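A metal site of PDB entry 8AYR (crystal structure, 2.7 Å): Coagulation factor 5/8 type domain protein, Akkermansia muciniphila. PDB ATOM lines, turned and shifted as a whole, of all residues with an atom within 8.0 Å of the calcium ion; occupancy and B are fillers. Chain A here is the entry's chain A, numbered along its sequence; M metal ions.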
ATOM      1  N   GLY A 382     -29.677 -13.516   8.993  1.00  0.00           N
ATOM      2  CA  GLY A 382     -30.310 -14.804   9.159  1.00  0.00           C
ATOM      3  C   GLY A 382     -29.338 -15.966   9.051  1.00  0.00           C
ATOM      4  O   GLY A 382     -28.165 -15.801   8.704  1.00  0.00           O
ATOM      5  N   ALA A 383     -29.839 -17.162   9.336  1.00  0.00           N
ATOM      6  CA  ALA A 383     -29.000 -18.354   9.360  1.00  0.00           C
ATOM      7  C   ALA A 383     -28.328 -18.584   8.008  1.00  0.00           C
ATOM      8  O   ALA A 383     -27.123 -18.851   7.930  1.00  0.00           O
ATOM      9  CB  ALA A 383     -29.825 -19.576   9.774  1.00  0.00           C
ATOM     10  N   GLU A 384     -29.098 -18.462   6.921  1.00  0.00           N
ATOM     11  CA  GLU A 384     -28.627 -18.634   5.549  1.00  0.00           C
ATOM     12  C   GLU A 384     -27.276 -17.977   5.295  1.00  0.00           C
ATOM     13  O   GLU A 384     -26.491 -18.455   4.463  1.00  0.00           O
ATOM     14  CB  GLU A 384     -29.669 -18.081   4.571  1.00  0.00           C
ATOM     15  CG  GLU A 384     -29.898 -16.579   4.708  1.00  0.00           C
ATOM     16  CD  GLU A 384     -30.954 -16.049   3.760  1.00  0.00           C
ATOM     17  OE1 GLU A 384     -31.560 -16.847   3.009  1.00  0.00           O
ATOM     18  OE2 GLU A 384     -31.161 -14.810   3.752  1.00  0.00           O
ATOM     19  N   GLN A 385     -26.994 -16.903   6.021  1.00  0.00           N
ATOM     20  CA  GLN A 385     -25.792 -16.103   5.825  1.00  0.00           C
ATOM     21  C   GLN A 385     -24.507 -16.862   6.154  1.00  0.00           C
ATOM     22  O   GLN A 385     -23.421 -16.284   5.973  1.00  0.00           O
ATOM     23  CB  GLN A 385     -25.865 -14.843   6.683  1.00  0.00           C
ATOM     24  CG  GLN A 385     -27.077 -13.947   6.415  1.00  0.00           C
ATOM     25  CD  GLN A 385     -27.036 -13.260   5.065  1.00  0.00           C
ATOM     26  OE1 GLN A 385     -25.986 -12.808   4.619  1.00  0.00           O
ATOM     27  NE2 GLN A 385     -28.198 -13.167   4.427  1.00  0.00           N
ATOM     28  N   VAL A 386     -24.571 -18.107   6.629  1.00  0.00           N
ATOM     29  CA  VAL A 386     -23.353 -18.852   6.938  1.00  0.00           C
ATOM     30  C   VAL A 386     -22.949 -19.814   5.818  1.00  0.00           C
ATOM     31  O   VAL A 386     -21.909 -20.476   5.934  1.00  0.00           O
ATOM     32  CB  VAL A 386     -23.484 -19.638   8.263  1.00  0.00           C
ATOM     33  CG1 VAL A 386     -23.751 -18.690   9.423  1.00  0.00           C
ATOM     34  CG2 VAL A 386     -24.567 -20.707   8.151  1.00  0.00           C
ATOM     35  N   LEU A 387     -23.735 -19.903   4.747  1.00  0.00           N
ATOM     36  CA  LEU A 387     -23.469 -20.881   3.699  1.00  0.00           C
ATOM     37  C   LEU A 387     -22.528 -20.390   2.608  1.00  0.00           C
ATOM     38  O   LEU A 387     -21.968 -21.205   1.880  1.00  0.00           O
ATOM     39  CB  LEU A 387     -24.788 -21.346   3.074  1.00  0.00           C
ATOM     40  CG  LEU A 387     -25.658 -22.207   3.985  1.00  0.00           C
ATOM     41  CD1 LEU A 387     -27.035 -22.390   3.395  1.00  0.00           C
ATOM     42  CD2 LEU A 387     -24.991 -23.554   4.187  1.00  0.00           C
ATOM     43  N   ASP A 388     -22.353 -19.077   2.469  1.00  0.00           N
ATOM     44  CA  ASP A 388     -21.496 -18.557   1.417  1.00  0.00           C
ATOM     45  C   ASP A 388     -20.025 -18.516   1.802  1.00  0.00           C
ATOM     46  O   ASP A 388     -19.209 -17.992   1.047  1.00  0.00           O
ATOM     47  CB  ASP A 388     -21.961 -17.149   1.004  1.00  0.00           C
ATOM     48  CG  ASP A 388     -21.974 -16.179   2.162  1.00  0.00           C
ATOM     49  OD1 ASP A 388     -21.673 -16.606   3.292  1.00  0.00           O
ATOM     50  OD2 ASP A 388     -22.311 -14.995   1.929  1.00  0.00           O
ATOM     51  N   ARG A 389     -19.675 -19.021   2.988  1.00  0.00           N
ATOM     52  CA  ARG A 389     -18.296 -19.107   3.474  1.00  0.00           C
ATOM     53  C   ARG A 389     -17.613 -17.751   3.576  1.00  0.00           C
ATOM     54  O   ARG A 389     -16.496 -17.659   4.096  1.00  0.00           O
ATOM     55  CB  ARG A 389     -17.452 -20.033   2.599  1.00  0.00           C
ATOM     56  CG  ARG A 389     -17.779 -21.515   2.696  1.00  0.00           C
ATOM     57  CD  ARG A 389     -16.718 -22.308   1.958  1.00  0.00           C
ATOM     58  NE  ARG A 389     -15.423 -22.110   2.604  1.00  0.00           N
ATOM     59  CZ  ARG A 389     -14.259 -22.510   2.116  1.00  0.00           C
ATOM     60  NH1 ARG A 389     -14.172 -23.146   0.959  1.00  0.00           N
ATOM     61  NH2 ARG A 389     -13.146 -22.248   2.810  1.00  0.00           N
ATOM     62  N   LYS A 390     -18.256 -16.692   3.089  1.00  0.00           N
ATOM     63  CA  LYS A 390     -17.611 -15.386   3.147  1.00  0.00           C
ATOM     64  C   LYS A 390     -17.621 -14.870   4.570  1.00  0.00           C
ATOM     65  O   LYS A 390     -18.644 -14.934   5.270  1.00  0.00           O
ATOM     66  CB  LYS A 390     -18.298 -14.395   2.205  1.00  0.00           C
ATOM     67  CG  LYS A 390     -18.158 -14.742   0.718  1.00  0.00           C
ATOM     68  CD  LYS A 390     -18.516 -13.557  -0.176  1.00  0.00           C
ATOM     69  CE  LYS A 390     -19.994 -13.249  -0.165  1.00  0.00           C
ATOM     70  NZ  LYS A 390     -20.325 -12.136  -1.089  1.00  0.00           N
ATOM     71  N   ARG A 391     -16.478 -14.373   5.016  1.00  0.00           N
ATOM     72  CA  ARG A 391     -16.325 -13.892   6.378  1.00  0.00           C
ATOM     73  C   ARG A 391     -17.011 -12.555   6.608  1.00  0.00           C
ATOM     74  O   ARG A 391     -17.217 -12.164   7.761  1.00  0.00           O
ATOM     75  CB  ARG A 391     -14.830 -13.848   6.709  1.00  0.00           C
ATOM     76  CG  ARG A 391     -14.432 -13.562   8.138  1.00  0.00           C
ATOM     77  CD  ARG A 391     -14.038 -12.117   8.273  1.00  0.00           C
ATOM     78  NE  ARG A 391     -12.994 -11.802   7.293  1.00  0.00           N
ATOM     79  CZ  ARG A 391     -12.685 -10.572   6.905  1.00  0.00           C
ATOM     80  NH1 ARG A 391     -13.313  -9.520   7.398  1.00  0.00           N
ATOM     81  NH2 ARG A 391     -11.735 -10.409   5.993  1.00  0.00           N
ATOM     82  N   THR A 392     -17.398 -11.850   5.537  1.00  0.00           N
ATOM     83  CA  THR A 392     -18.060 -10.554   5.595  1.00  0.00           C
ATOM     84  C   THR A 392     -19.570 -10.634   5.787  1.00  0.00           C
ATOM     85  O   THR A 392     -20.190  -9.611   6.096  1.00  0.00           O
ATOM     86  CB  THR A 392     -17.744  -9.751   4.329  1.00  0.00           C
ATOM     87  OG1 THR A 392     -18.340  -8.451   4.435  1.00  0.00           O
ATOM     88  CG2 THR A 392     -18.275 -10.464   3.097  1.00  0.00           C
ATOM     89  N   THR A 393     -20.180 -11.798   5.572  1.00  0.00           N
ATOM     90  CA  THR A 393     -21.610 -12.009   5.750  1.00  0.00           C
ATOM     91  C   THR A 393     -21.820 -12.998   6.891  1.00  0.00           C
ATOM     92  O   THR A 393     -21.127 -14.011   6.962  1.00  0.00           O
ATOM     93  CB  THR A 393     -22.261 -12.522   4.472  1.00  0.00           C
ATOM     94  OG1 THR A 393     -21.643 -13.765   4.096  1.00  0.00           O
ATOM     95  CG2 THR A 393     -22.104 -11.523   3.343  1.00  0.00           C
ATOM     96  N   TYR A 394     -22.759 -12.704   7.777  1.00  0.00           N
ATOM     97  CA  TYR A 394     -22.831 -13.463   9.015  1.00  0.00           C
ATOM     98  C   TYR A 394     -24.234 -13.484   9.600  1.00  0.00           C
ATOM     99  O   TYR A 394     -25.071 -12.623   9.328  1.00  0.00           O
ATOM    100  CB  TYR A 394     -21.829 -12.918  10.046  1.00  0.00           C
ATOM    101  CG  TYR A 394     -21.898 -11.408  10.194  1.00  0.00           C
ATOM    102  CD1 TYR A 394     -21.109 -10.587   9.405  1.00  0.00           C
ATOM    103  CD2 TYR A 394     -22.766 -10.809  11.098  1.00  0.00           C
ATOM    104  CE1 TYR A 394     -21.157  -9.206   9.515  1.00  0.00           C
ATOM    105  CE2 TYR A 394     -22.827  -9.431  11.214  1.00  0.00           C
ATOM    106  CZ  TYR A 394     -22.025  -8.636  10.423  1.00  0.00           C
ATOM    107  OH  TYR A 394     -22.073  -7.255  10.533  1.00  0.00           O
ATOM    108  N   TRP A 395     -24.472 -14.507  10.416  1.00  0.00           N
ATOM    109  CA  TRP A 395     -25.648 -14.653  11.265  1.00  0.00           C
ATOM    110  C   TRP A 395     -25.354 -14.142  12.662  1.00  0.00           C
ATOM    111  O   TRP A 395     -24.264 -14.368  13.188  1.00  0.00           O
ATOM    112  CB  TRP A 395     -26.077 -16.125  11.351  1.00  0.00           C
ATOM    113  CG  TRP A 395     -27.067 -16.367  12.440  1.00  0.00           C
ATOM    114  CD1 TRP A 395     -28.364 -15.946  12.475  1.00  0.00           C
ATOM    115  CD2 TRP A 395     -26.826 -17.042  13.685  1.00  0.00           C
ATOM    116  NE1 TRP A 395     -28.952 -16.345  13.652  1.00  0.00           N
ATOM    117  CE2 TRP A 395     -28.031 -17.023  14.408  1.00  0.00           C
ATOM    118  CE3 TRP A 395     -25.709 -17.671  14.244  1.00  0.00           C
ATOM    119  CZ2 TRP A 395     -28.149 -17.608  15.666  1.00  0.00           C
ATOM    120  CZ3 TRP A 395     -25.833 -18.248  15.493  1.00  0.00           C
ATOM    121  CH2 TRP A 395     -27.051 -18.218  16.191  1.00  0.00           C
ATOM    122  N   ALA A 422     -16.791 -20.469  11.490  1.00  0.00           N
ATOM    123  CA  ALA A 422     -16.116 -19.172  11.446  1.00  0.00           C
ATOM    124  C   ALA A 422     -17.069 -18.069  11.883  1.00  0.00           C
ATOM    125  O   ALA A 422     -18.264 -18.107  11.559  1.00  0.00           O
ATOM    126  CB  ALA A 422     -15.557 -18.875  10.053  1.00  0.00           C
ATOM    127  N   LEU A 482     -21.930 -16.040  13.724  1.00  0.00           N
ATOM    128  CA  LEU A 482     -21.167 -16.937  12.874  1.00  0.00           C
ATOM    129  C   LEU A 482     -21.259 -16.467  11.427  1.00  0.00           C
ATOM    130  O   LEU A 482     -22.325 -16.049  10.968  1.00  0.00           O
ATOM    131  CB  LEU A 482     -21.667 -18.393  12.968  1.00  0.00           C
ATOM    132  CG  LEU A 482     -21.102 -19.280  14.085  1.00  0.00           C
ATOM    133  CD1 LEU A 482     -21.587 -18.857  15.446  1.00  0.00           C
ATOM    134  CD2 LEU A 482     -21.440 -20.738  13.817  1.00  0.00           C
ATOM    135  N   CYS A 483     -20.129 -16.543  10.720  1.00  0.00           N
ATOM    136  CA  CYS A 483     -20.080 -16.176   9.310  1.00  0.00           C
ATOM    137  C   CYS A 483     -19.876 -17.371   8.387  1.00  0.00           C
ATOM    138  O   CYS A 483     -20.042 -17.219   7.169  1.00  0.00           O
ATOM    139  CB  CYS A 483     -18.963 -15.143   9.057  1.00  0.00           C
ATOM    140  SG  CYS A 483     -17.255 -15.750   9.281  1.00  0.00           S
ATOM    141  N   GLU A 484     -19.521 -18.534   8.917  1.00  0.00           N
ATOM    142  CA  GLU A 484     -19.357 -19.725   8.087  1.00  0.00           C
ATOM    143  C   GLU A 484     -19.703 -20.976   8.876  1.00  0.00           C
ATOM    144  O   GLU A 484     -19.256 -21.136  10.014  1.00  0.00           O
ATOM    145  CB  GLU A 484     -17.927 -19.850   7.561  1.00  0.00           C
ATOM    146  CG  GLU A 484     -17.735 -21.084   6.684  1.00  0.00           C
ATOM    147  CD  GLU A 484     -16.304 -21.264   6.222  1.00  0.00           C
ATOM    148  OE1 GLU A 484     -15.424 -20.467   6.637  1.00  0.00           O
ATOM    149  OE2 GLU A 484     -16.065 -22.216   5.441  1.00  0.00           O
ATOM    150  N   VAL A 485     -20.511 -21.848   8.259  1.00  0.00           N
ATOM    151  CA  VAL A 485     -20.696 -23.235   8.688  1.00  0.00           C
ATOM    152  C   VAL A 485     -20.616 -24.091   7.434  1.00  0.00           C
ATOM    153  O   VAL A 485     -21.521 -24.036   6.585  1.00  0.00           O
ATOM    154  CB  VAL A 485     -22.039 -23.454   9.402  1.00  0.00           C
ATOM    155  CG1 VAL A 485     -22.175 -24.912   9.797  1.00  0.00           C
ATOM    156  CG2 VAL A 485     -22.150 -22.574  10.633  1.00  0.00           C
HETATM  157 CA    CA M   1     -21.122 -15.687   5.348  1.00  0.00          CA
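NE2 of Gln 385 sits at hydrogen-bond distance from OE2 of Glu 384.
N of Cys 483 is in hydrogen-bond range of O of Ala 422, 2.6 Å away.
The calcium ion is bound by OD1 of Asp 388 (2.3 Å), O of Thr 393 (2.3 Å), OG1 of Thr 393 (2.4 Å), O of Gln 385 (2.5 Å), O of Lys 390 (2.6 Å) and O of Cys 483 (2.6 Å).
The nearest printed residue that does not touch the calcium ion is Tyr 394 (4.2 Å).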
